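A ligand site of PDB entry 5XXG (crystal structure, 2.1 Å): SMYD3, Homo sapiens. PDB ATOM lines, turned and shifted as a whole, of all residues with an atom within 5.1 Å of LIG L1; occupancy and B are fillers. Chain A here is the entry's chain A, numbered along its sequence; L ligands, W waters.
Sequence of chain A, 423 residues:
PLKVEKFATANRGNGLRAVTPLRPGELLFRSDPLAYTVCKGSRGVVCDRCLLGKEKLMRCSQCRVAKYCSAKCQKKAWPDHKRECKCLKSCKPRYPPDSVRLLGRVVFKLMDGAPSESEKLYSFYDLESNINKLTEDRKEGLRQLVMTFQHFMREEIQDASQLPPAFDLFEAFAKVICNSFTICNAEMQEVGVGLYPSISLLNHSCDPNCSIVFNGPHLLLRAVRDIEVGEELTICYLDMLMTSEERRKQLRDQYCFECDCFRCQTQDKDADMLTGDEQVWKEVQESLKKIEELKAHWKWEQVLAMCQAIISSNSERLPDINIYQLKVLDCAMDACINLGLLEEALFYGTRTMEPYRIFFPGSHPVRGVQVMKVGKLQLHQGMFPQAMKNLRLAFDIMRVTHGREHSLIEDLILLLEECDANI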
ATOM      1  N   ASN A  11      12.660  25.145  21.576  1.00  0.00           N
ATOM      2  CA  ASN A  11      12.229  25.051  20.185  1.00  0.00           C
ATOM      3  C   ASN A  11      13.272  25.534  19.176  1.00  0.00           C
ATOM      4  O   ASN A  11      12.911  25.780  18.017  1.00  0.00           O
ATOM      5  CB  ASN A  11      10.914  25.846  19.965  1.00  0.00           C
ATOM      6  CG  ASN A  11      11.018  27.307  20.390  1.00  0.00           C
ATOM      7  OD1 ASN A  11      12.073  27.943  20.269  1.00  0.00           O
ATOM      8  ND2 ASN A  11       9.922  27.853  20.877  1.00  0.00           N
ATOM      9  N   ARG A  12      14.543  25.675  19.576  1.00  0.00           N
ATOM     10  CA  ARG A  12      15.634  26.074  18.685  1.00  0.00           C
ATOM     11  C   ARG A  12      16.784  25.071  18.720  1.00  0.00           C
ATOM     12  O   ARG A  12      17.937  25.461  18.545  1.00  0.00           O
ATOM     13  CB  ARG A  12      16.175  27.459  19.049  1.00  0.00           C
ATOM     14  CG  ARG A  12      15.175  28.560  19.275  1.00  0.00           C
ATOM     15  CD  ARG A  12      15.849  29.737  19.973  1.00  0.00           C
ATOM     16  NE  ARG A  12      14.909  30.821  20.185  1.00  0.00           N
ATOM     17  CZ  ARG A  12      15.168  31.909  20.915  1.00  0.00           C
ATOM     18  NH1 ARG A  12      16.358  32.054  21.492  1.00  0.00           N
ATOM     19  NH2 ARG A  12      14.252  32.845  21.058  1.00  0.00           N
ATOM     20  N   GLY A  13      16.492  23.792  18.983  1.00  0.00           N
ATOM     21  CA  GLY A  13      17.555  22.804  19.106  1.00  0.00           C
ATOM     22  C   GLY A  13      18.459  23.073  20.294  1.00  0.00           C
ATOM     23  O   GLY A  13      18.012  23.555  21.348  1.00  0.00           O
ATOM     24  N   ASN A  14      19.741  22.762  20.139  1.00  0.00           N
ATOM     25  CA  ASN A  14      20.721  23.070  21.175  1.00  0.00           C
ATOM     26  C   ASN A  14      21.116  24.548  21.122  1.00  0.00           C
ATOM     27  O   ASN A  14      20.997  25.194  20.079  1.00  0.00           O
ATOM     28  CB  ASN A  14      21.970  22.204  21.019  1.00  0.00           C
ATOM     29  CG  ASN A  14      21.647  20.748  21.166  1.00  0.00           C
ATOM     30  OD1 ASN A  14      20.958  20.360  22.104  1.00  0.00           O
ATOM     31  ND2 ASN A  14      22.099  19.943  20.226  1.00  0.00           N
ATOM     32  N   GLY A  15      21.576  25.056  22.269  1.00  0.00           N
ATOM     33  CA  GLY A  15      21.985  26.452  22.414  1.00  0.00           C
ATOM     34  C   GLY A  15      23.037  26.618  23.504  1.00  0.00           C
ATOM     35  O   GLY A  15      23.480  25.655  24.117  1.00  0.00           O
ATOM     36  N   TYR A 122      31.030  21.130  21.519  1.00  0.00           N
ATOM     37  CA  TYR A 122      30.159  20.723  20.419  1.00  0.00           C
ATOM     38  C   TYR A 122      31.075  20.364  19.261  1.00  0.00           C
ATOM     39  O   TYR A 122      32.021  21.110  18.992  1.00  0.00           O
ATOM     40  CB  TYR A 122      29.232  21.880  20.029  1.00  0.00           C
ATOM     41  CG  TYR A 122      27.838  21.535  19.486  1.00  0.00           C
ATOM     42  CD1 TYR A 122      27.000  20.631  20.135  1.00  0.00           C
ATOM     43  CD2 TYR A 122      27.344  22.187  18.353  1.00  0.00           C
ATOM     44  CE1 TYR A 122      25.718  20.364  19.658  1.00  0.00           C
ATOM     45  CE2 TYR A 122      26.078  21.927  17.858  1.00  0.00           C
ATOM     46  CZ  TYR A 122      25.269  21.018  18.516  1.00  0.00           C
ATOM     47  OH  TYR A 122      24.015  20.763  18.017  1.00  0.00           O
ATOM     48  N   ASP A 126      28.166  16.766  15.895  1.00  0.00           N
ATOM     49  CA  ASP A 126      26.971  17.252  16.586  1.00  0.00           C
ATOM     50  C   ASP A 126      26.183  18.274  15.785  1.00  0.00           C
ATOM     51  O   ASP A 126      25.026  18.549  16.127  1.00  0.00           O
ATOM     52  CB  ASP A 126      27.363  17.894  17.913  1.00  0.00           C
ATOM     53  CG  ASP A 126      27.978  16.937  18.891  1.00  0.00           C
ATOM     54  OD1 ASP A 126      27.480  15.790  18.980  1.00  0.00           O
ATOM     55  OD2 ASP A 126      28.925  17.341  19.600  1.00  0.00           O
ATOM     56  N   LEU A 127      26.798  18.886  14.782  1.00  0.00           N
ATOM     57  CA  LEU A 127      26.244  20.091  14.168  1.00  0.00           C
ATOM     58  C   LEU A 127      24.857  19.843  13.582  1.00  0.00           C
ATOM     59  O   LEU A 127      24.583  18.773  13.025  1.00  0.00           O
ATOM     60  CB  LEU A 127      27.172  20.616  13.078  1.00  0.00           C
ATOM     61  CG  LEU A 127      28.524  21.130  13.576  1.00  0.00           C
ATOM     62  CD1 LEU A 127      29.405  21.574  12.386  1.00  0.00           C
ATOM     63  CD2 LEU A 127      28.329  22.257  14.587  1.00  0.00           C
ATOM     64  N   GLU A 128      23.989  20.852  13.699  1.00  0.00           N
ATOM     65  CA  GLU A 128      22.694  20.779  13.039  1.00  0.00           C
ATOM     66  C   GLU A 128      22.870  20.706  11.524  1.00  0.00           C
ATOM     67  O   GLU A 128      23.685  21.424  10.944  1.00  0.00           O
ATOM     68  CB  GLU A 128      21.859  22.014  13.415  1.00  0.00           C
ATOM     69  CG  GLU A 128      20.508  22.096  12.698  1.00  0.00           C
ATOM     70  CD  GLU A 128      19.534  21.052  13.205  1.00  0.00           C
ATOM     71  OE1 GLU A 128      18.994  21.248  14.318  1.00  0.00           O
ATOM     72  OE2 GLU A 128      19.308  20.032  12.503  1.00  0.00           O
ATOM     73  N   ASN A 130      19.725  20.283   9.554  1.00  0.00           N
ATOM     74  CA  ASN A 130      18.406  20.696   9.036  1.00  0.00           C
ATOM     75  C   ASN A 130      17.930  19.863   7.842  1.00  0.00           C
ATOM     76  O   ASN A 130      17.151  20.347   7.016  1.00  0.00           O
ATOM     77  CB  ASN A 130      18.410  22.189   8.677  1.00  0.00           C
ATOM     78  CG  ASN A 130      18.280  23.074   9.919  1.00  0.00           C
ATOM     79  OD1 ASN A 130      17.444  22.834  10.781  1.00  0.00           O
ATOM     80  ND2 ASN A 130      19.121  24.096  10.013  1.00  0.00           N
ATOM     81  N   CYS A 178      24.669  25.763   7.246  1.00  0.00           N
ATOM     82  CA  CYS A 178      24.083  26.501   8.344  1.00  0.00           C
ATOM     83  C   CYS A 178      25.014  26.617   9.544  1.00  0.00           C
ATOM     84  O   CYS A 178      24.563  27.002  10.628  1.00  0.00           O
ATOM     85  CB  CYS A 178      22.745  25.876   8.732  1.00  0.00           C
ATOM     86  SG  CYS A 178      22.854  24.234   9.473  1.00  0.00           S
ATOM     87  N   ASN A 179      26.295  26.311   9.367  1.00  0.00           N
ATOM     88  CA  ASN A 179      27.276  26.531  10.434  1.00  0.00           C
ATOM     89  C   ASN A 179      28.577  27.178   9.978  1.00  0.00           C
ATOM     90  O   ASN A 179      29.493  27.279  10.791  1.00  0.00           O
ATOM     91  CB  ASN A 179      27.611  25.214  11.142  1.00  0.00           C
ATOM     92  CG  ASN A 179      26.418  24.633  11.890  1.00  0.00           C
ATOM     93  OD1 ASN A 179      26.042  25.148  12.936  1.00  0.00           O
ATOM     94  ND2 ASN A 179      25.814  23.584  11.338  1.00  0.00           N
ATOM     95  N   SER A 200      29.196  27.283  17.107  1.00  0.00           N
ATOM     96  CA  SER A 200      27.971  27.007  16.366  1.00  0.00           C
ATOM     97  C   SER A 200      26.803  26.687  17.285  1.00  0.00           C
ATOM     98  O   SER A 200      25.666  26.570  16.828  1.00  0.00           O
ATOM     99  CB  SER A 200      28.182  25.839  15.401  1.00  0.00           C
ATOM    100  OG  SER A 200      28.870  26.251  14.244  1.00  0.00           O
ATOM    101  N   LEU A 201      27.048  26.518  18.585  1.00  0.00           N
ATOM    102  CA  LEU A 201      25.927  26.357  19.505  1.00  0.00           C
ATOM    103  C   LEU A 201      25.045  27.608  19.597  1.00  0.00           C
ATOM    104  O   LEU A 201      23.875  27.486  19.955  1.00  0.00           O
ATOM    105  CB  LEU A 201      26.420  25.993  20.906  1.00  0.00           C
ATOM    106  CG  LEU A 201      26.624  24.515  21.229  1.00  0.00           C
ATOM    107  CD1 LEU A 201      27.260  24.366  22.610  1.00  0.00           C
ATOM    108  CD2 LEU A 201      25.303  23.730  21.134  1.00  0.00           C
ATOM    109  N   LEU A 202      25.580  28.786  19.263  1.00  0.00           N
ATOM    110  CA  LEU A 202      24.839  30.030  19.475  1.00  0.00           C
ATOM    111  C   LEU A 202      23.708  30.160  18.476  1.00  0.00           C
ATOM    112  O   LEU A 202      23.937  30.191  17.262  1.00  0.00           O
ATOM    113  CB  LEU A 202      25.761  31.246  19.376  1.00  0.00           C
ATOM    114  CG  LEU A 202      26.838  31.411  20.466  1.00  0.00           C
ATOM    115  CD1 LEU A 202      28.106  31.943  19.876  1.00  0.00           C
ATOM    116  CD2 LEU A 202      26.355  32.330  21.597  1.00  0.00           C
ATOM    117  N   ASN A 203      22.484  30.286  18.989  1.00  0.00           N
ATOM    118  CA  ASN A 203      21.344  30.595  18.140  1.00  0.00           C
ATOM    119  C   ASN A 203      21.320  32.093  17.773  1.00  0.00           C
ATOM    120  O   ASN A 203      22.045  32.914  18.351  1.00  0.00           O
ATOM    121  CB  ASN A 203      20.054  30.157  18.833  1.00  0.00           C
ATOM    122  CG  ASN A 203      19.876  28.659  18.768  1.00  0.00           C
ATOM    123  OD1 ASN A 203      20.109  28.044  17.734  1.00  0.00           O
ATOM    124  ND2 ASN A 203      19.500  28.049  19.882  1.00  0.00           N
ATOM    125  N   HIS A 204      20.489  32.432  16.784  1.00  0.00           N
ATOM    126  CA  HIS A 204      20.387  33.774  16.201  1.00  0.00           C
ATOM    127  C   HIS A 204      19.394  34.646  16.959  1.00  0.00           C
ATOM    128  O   HIS A 204      18.359  34.175  17.449  1.00  0.00           O
ATOM    129  CB  HIS A 204      19.935  33.704  14.747  1.00  0.00           C
ATOM    130  CG  HIS A 204      19.466  35.033  14.209  1.00  0.00           C
ATOM    131  ND1 HIS A 204      20.321  35.938  13.623  1.00  0.00           N
ATOM    132  CD2 HIS A 204      18.225  35.586  14.141  1.00  0.00           C
ATOM    133  CE1 HIS A 204      19.639  37.001  13.236  1.00  0.00           C
ATOM    134  NE2 HIS A 204      18.368  36.827  13.548  1.00  0.00           N
ATOM    135  N   SER A 205      19.685  35.932  16.990  1.00  0.00           N
ATOM    136  CA  SER A 205      18.727  36.962  17.392  1.00  0.00           C
ATOM    137  C   SER A 205      18.956  38.193  16.520  1.00  0.00           C
ATOM    138  O   SER A 205      20.103  38.581  16.262  1.00  0.00           O
ATOM    139  CB  SER A 205      18.870  37.334  18.876  1.00  0.00           C
ATOM    140  OG  SER A 205      18.014  38.414  19.177  1.00  0.00           O
ATOM    141  N   TYR A 237      23.241  36.496  13.141  1.00  0.00           N
ATOM    142  CA  TYR A 237      23.894  35.820  12.015  1.00  0.00           C
ATOM    143  C   TYR A 237      24.113  36.735  10.818  1.00  0.00           C
ATOM    144  O   TYR A 237      24.902  36.398   9.928  1.00  0.00           O
ATOM    145  CB  TYR A 237      23.045  34.627  11.555  1.00  0.00           C
ATOM    146  CG  TYR A 237      22.955  33.456  12.506  1.00  0.00           C
ATOM    147  CD1 TYR A 237      23.634  33.445  13.724  1.00  0.00           C
ATOM    148  CD2 TYR A 237      22.209  32.321  12.166  1.00  0.00           C
ATOM    149  CE1 TYR A 237      23.550  32.347  14.586  1.00  0.00           C
ATOM    150  CE2 TYR A 237      22.121  31.239  13.014  1.00  0.00           C
ATOM    151  CZ  TYR A 237      22.793  31.257  14.225  1.00  0.00           C
ATOM    152  OH  TYR A 237      22.696  30.158  15.068  1.00  0.00           O
ATOM    153  N   TYR A 255      19.388  28.991   6.908  1.00  0.00           N
ATOM    154  CA  TYR A 255      19.299  28.446   8.260  1.00  0.00           C
ATOM    155  C   TYR A 255      18.011  27.698   8.567  1.00  0.00           C
ATOM    156  O   TYR A 255      17.892  27.173   9.677  1.00  0.00           O
ATOM    157  CB  TYR A 255      19.493  29.562   9.291  1.00  0.00           C
ATOM    158  CG  TYR A 255      20.881  30.201   9.211  1.00  0.00           C
ATOM    159  CD1 TYR A 255      21.993  29.553   9.722  1.00  0.00           C
ATOM    160  CD2 TYR A 255      21.059  31.431   8.582  1.00  0.00           C
ATOM    161  CE1 TYR A 255      23.258  30.118   9.633  1.00  0.00           C
ATOM    162  CE2 TYR A 255      22.309  32.015   8.497  1.00  0.00           C
ATOM    163  CZ  TYR A 255      23.405  31.360   9.026  1.00  0.00           C
ATOM    164  OH  TYR A 255      24.642  31.943   8.923  1.00  0.00           O
ATOM    165  N   CYS A 256      17.072  27.623   7.631  1.00  0.00           N
ATOM    166  CA  CYS A 256      15.824  26.864   7.779  1.00  0.00           C
ATOM    167  C   CYS A 256      15.069  27.181   9.067  1.00  0.00           C
ATOM    168  O   CYS A 256      14.622  26.278   9.789  1.00  0.00           O
ATOM    169  CB  CYS A 256      16.073  25.346   7.684  1.00  0.00           C
ATOM    170  SG  CYS A 256      16.620  24.758   6.071  1.00  0.00           S
ATOM    171  N   PHE A 257      14.922  28.475   9.381  1.00  0.00           N
ATOM    172  CA  PHE A 257      13.965  28.807  10.437  1.00  0.00           C
ATOM    173  C   PHE A 257      13.307  30.146  10.156  1.00  0.00           C
ATOM    174  O   PHE A 257      13.776  30.944   9.338  1.00  0.00           O
ATOM    175  CB  PHE A 257      14.620  28.772  11.838  1.00  0.00           C
ATOM    176  CG  PHE A 257      15.510  29.962  12.156  1.00  0.00           C
ATOM    177  CD1 PHE A 257      15.000  31.090  12.792  1.00  0.00           C
ATOM    178  CD2 PHE A 257      16.858  29.940  11.824  1.00  0.00           C
ATOM    179  CE1 PHE A 257      15.816  32.173  13.096  1.00  0.00           C
ATOM    180  CE2 PHE A 257      17.682  31.020  12.123  1.00  0.00           C
ATOM    181  CZ  PHE A 257      17.151  32.146  12.768  1.00  0.00           C
ATOM    182  N   GLU A 258      12.185  30.366  10.843  1.00  0.00           N
ATOM    183  CA  GLU A 258      11.435  31.628  10.825  1.00  0.00           C
ATOM    184  C   GLU A 258      11.688  32.356  12.141  1.00  0.00           C
ATOM    185  O   GLU A 258      11.578  31.755  13.212  1.00  0.00           O
ATOM    186  CB  GLU A 258       9.939  31.363  10.649  1.00  0.00           C
ATOM    187  CG  GLU A 258       9.626  30.097   9.862  1.00  0.00           C
ATOM    188  CD  GLU A 258       9.792  30.323   8.371  1.00  0.00           C
ATOM    189  OE1 GLU A 258      10.009  31.497   7.963  1.00  0.00           O
ATOM    190  OE2 GLU A 258       9.745  29.335   7.618  1.00  0.00           O
HETATM  191  N1  LIG L   1      20.353  25.274  17.397  1.00  0.00           N
HETATM  192  C1  LIG L   1      21.574  24.902  16.698  1.00  0.00           C
HETATM  193  C2  LIG L   1      21.968  23.463  17.017  1.00  0.00           C
HETATM  194  O1  LIG L   1      21.147  22.725  17.542  1.00  0.00           O
HETATM  195  O2  LIG L   1      23.094  23.017  16.743  1.00  0.00           O
HETATM  196  C3  LIG L   1      22.697  25.855  17.080  1.00  0.00           C
HETATM  197  C4  LIG L   1      22.770  27.085  16.164  1.00  0.00           C
HETATM  198  S1  LIG L   1      23.312  26.588  14.511  1.00  0.00           S
HETATM  199  C5  LIG L   1      24.669  27.743  14.228  1.00  0.00           C
HETATM  200  C6  LIG L   1      22.051  27.330  13.427  1.00  0.00           C
HETATM  201  C7  LIG L   1      20.695  26.619  13.445  1.00  0.00           C
HETATM  202  O3  LIG L   1      20.061  26.730  14.710  1.00  0.00           O
HETATM  203  C8  LIG L   1      19.693  27.168  12.421  1.00  0.00           C
HETATM  204  O4  LIG L   1      19.860  26.581  11.143  1.00  0.00           O
HETATM  205  C9  LIG L   1      18.358  26.845  13.058  1.00  0.00           C
HETATM  206  O5  LIG L   1      18.031  25.468  12.893  1.00  0.00           O
HETATM  207  C10 LIG L   1      18.670  26.996  14.523  1.00  0.00           C
HETATM  208  N2  LIG L   1      18.417  28.383  14.982  1.00  0.00           N
HETATM  209  C11 LIG L   1      19.344  29.377  15.165  1.00  0.00           C
HETATM  210  N3  LIG L   1      18.685  30.484  15.611  1.00  0.00           N
HETATM  211  C12 LIG L   1      17.363  30.207  15.718  1.00  0.00           C
HETATM  212  C13 LIG L   1      16.270  30.953  16.116  1.00  0.00           C
HETATM  213  N4  LIG L   1      16.373  32.226  16.513  1.00  0.00           N
HETATM  214  N5  LIG L   1      15.028  30.353  16.091  1.00  0.00           N
HETATM  215  C14 LIG L   1      14.867  29.053  15.698  1.00  0.00           C
HETATM  216  N6  LIG L   1      15.961  28.314  15.316  1.00  0.00           N
HETATM  217  C15 LIG L   1      17.192  28.889  15.321  1.00  0.00           C
HETATM  218  C1  LG2 L   2      31.103  40.730   9.728  1.00  0.00           C
HETATM  219  C2  LG2 L   2      32.267  40.159   9.244  1.00  0.00           C
HETATM  220  C3  LG2 L   2      32.751  38.977   9.759  1.00  0.00           C
HETATM  221  C4  LG2 L   2      32.058  38.350  10.805  1.00  0.00           C
HETATM  222  C5  LG2 L   2      30.869  38.910  11.297  1.00  0.00           C
HETATM  223  C6  LG2 L   2      30.406  40.112  10.745  1.00  0.00           C
HETATM  224  C7  LG2 L   2      31.312  42.509   8.202  1.00  0.00           C
HETATM  225  C8  LG2 L   2      32.474  41.993   7.684  1.00  0.00           C
HETATM  226  C9  LG2 L   2      32.926  40.818   8.242  1.00  0.00           C
HETATM  227  C10 LG2 L   2      30.813  43.693   7.720  1.00  0.00           C
HETATM  228  C11 LG2 L   2      30.104  38.336  12.319  1.00  0.00           C
HETATM  229  C12 LG2 L   2      29.585  36.408  10.830  1.00  0.00           C
HETATM  230  C13 LG2 L   2      28.282  35.703  10.472  1.00  0.00           C
HETATM  231  C14 LG2 L   2      28.323  35.061  12.951  1.00  0.00           C
HETATM  232  C15 LG2 L   2      28.554  36.569  13.164  1.00  0.00           C
HETATM  233  C16 LG2 L   2      27.153  33.702  11.228  1.00  0.00           C
HETATM  234  C17 LG2 L   2      27.093  31.484  11.797  1.00  0.00           C
HETATM  235  C18 LG2 L   2      26.770  30.570  12.972  1.00  0.00           C
HETATM  236  C19 LG2 L   2      27.331  29.165  12.715  1.00  0.00           C
HETATM  237  C20 LG2 L   2      29.553  44.067   8.172  1.00  0.00           C
HETATM  238  C21 LG2 L   2      28.994  45.263   7.725  1.00  0.00           C
HETATM  239  C22 LG2 L   2      29.680  46.098   6.852  1.00  0.00           C
HETATM  240  C23 LG2 L   2      30.936  45.710   6.420  1.00  0.00           C
HETATM  241  C24 LG2 L   2      31.519  44.518   6.844  1.00  0.00           C
HETATM  242  N1  LG2 L   2      30.651  41.888   9.199  1.00  0.00           N
HETATM  243  N2  LG2 L   2      29.454  37.160  12.106  1.00  0.00           N
HETATM  244  N3  LG2 L   2      27.891  34.774  11.554  1.00  0.00           N
HETATM  245  O1  LG2 L   2      29.958  38.975  13.356  1.00  0.00           O
HETATM  246  O2  LG2 L   2      26.818  33.548  10.051  1.00  0.00           O
HETATM  247  O3  LG2 L   2      26.744  32.813  12.168  1.00  0.00           O
HETATM  248  O   HOH W   1      15.589  24.950  11.775  1.00  0.00           O
HETATM  249  O   HOH W   2      14.243  34.258  16.999  1.00  0.00           O
HETATM  250  O   HOH W   3      14.604  25.847  14.478  1.00  0.00           O
HETATM  251  O   HOH W   4      24.826  23.256  14.925  1.00  0.00           O
HETATM  252  O   HOH W   5      18.571  23.800  15.599  1.00  0.00           O
HETATM  253  O   HOH W   6      11.728  28.551  16.946  1.00  0.00           O
HETATM  254  O   HOH W   7      20.604  20.134  16.761  1.00  0.00           O
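The backbone carbonyl oxygen (O) of Tyr 255 lies within hydrogen-bond range of the side-chain amide nitrogen (ND2) of Asn 130 (3.3 Å). ND2 of Asn 203 sits at hydrogen-bond distance from O of Arg 12, at 3.3 Å. OH of Tyr 122 is in hydrogen-bond range of ND2 of Asn 14, at 3.0 Å. The side-chain hydroxyl of Tyr 122 lies within hydrogen-bond range of the backbone carbonyl oxygen of Asp 126 (3.1 Å). The side-chain amide nitrogen (ND2) of Asn 130 sits at hydrogen-bond distance from the side-chain sulfur (SG) of Cys 178 (3.8 Å). The side-chain hydroxyl (OG) of Ser 200 sits at hydrogen-bond distance from the side-chain amide oxygen (OD1) of Asn 179, 3.3 Å away. The side-chain amide nitrogen of Asn 179 sits at hydrogen-bond distance from the side-chain sulfur of Cys 178 (3.6 Å). OH of Tyr 237 sits at hydrogen-bond distance from O of Leu 202.
The side-chain amide oxygen of Asn 179 lies close to a sulfur (S1) of LIG L1, 3.5 Å away. The backbone carbonyl oxygen (O) of Ser 200 sits close to a sulfur (S1) of LIG L1 (3.3 Å). OH of Tyr 237 sits close to S1 of LIG L1 (3.7 Å). Merely in contact with LIG L1: Gly 13 (3.9 Å), Glu 128 (3.7 Å), Cys 178 (3.7 Å), Leu 201 (3.5 Å), Leu 202 (3.5 Å) and Phe 257 (3.3 Å). Of the 23 residues printed, 16 come within 4 Å of LIG L1.
The backbone carbonyl oxygen of Tyr 255 sits at hydrogen-bond distance from an oxygen (O4) of LIG L1 (2.5 Å). The backbone carbonyl oxygen (O) of Arg 12 is in hydrogen-bond range of a nitrogen (N1) of LIG L1 (2.7 Å). OH of Tyr 122 lies within hydrogen-bond range of O2 of LIG L1 (2.7 Å). An oxygen (O1) of LIG L1 sits at hydrogen-bond distance from the backbone NH (N) of Asn 14 (3.0 Å). The backbone carbonyl oxygen of Asn 14 sits at hydrogen-bond distance from a nitrogen (N1) of LIG L1, at 2.8 Å. OD1 of Asn 203 sits at hydrogen-bond distance from N1 of LIG L1 (2.8 Å). The side-chain amide nitrogen (ND2) of Asn 130 is in hydrogen-bond range of an oxygen (O4) of LIG L1, 2.8 Å away. The backbone NH (N) of His 204 sits at hydrogen-bond distance from a nitrogen (N3) of LIG L1 (2.9 Å). A nitrogen (N4) of LIG L1 lies within hydrogen-bond range of the backbone carbonyl oxygen (O) of His 204, 2.9 Å away. O2 of LG2 L2 is in hydrogen-bond range of OH of Tyr 255, 2.9 Å away.
Water W4 lies within hydrogen-bond range of O2 of LIG L1 (2.5 Å), N of Glu 128 (2.8 Å) and OD1 of Asn 179 (3.0 Å). Water W1 lies within hydrogen-bond range of O of Cys 256 (2.6 Å), O5 of LIG L1 (2.7 Å) and OD1 of Asn 130 (3.0 Å). Water W7 bridges an oxygen (O1) of LIG L1 (2.8 Å) and the side-chain carboxylate (OE1) of Glu 128 (3.1 Å). Water W5 lies within hydrogen-bond range of OE1 of Glu 128 (2.9 Å), N1 of LIG L1 (2.9 Å) and O of Arg 12 (3.4 Å).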
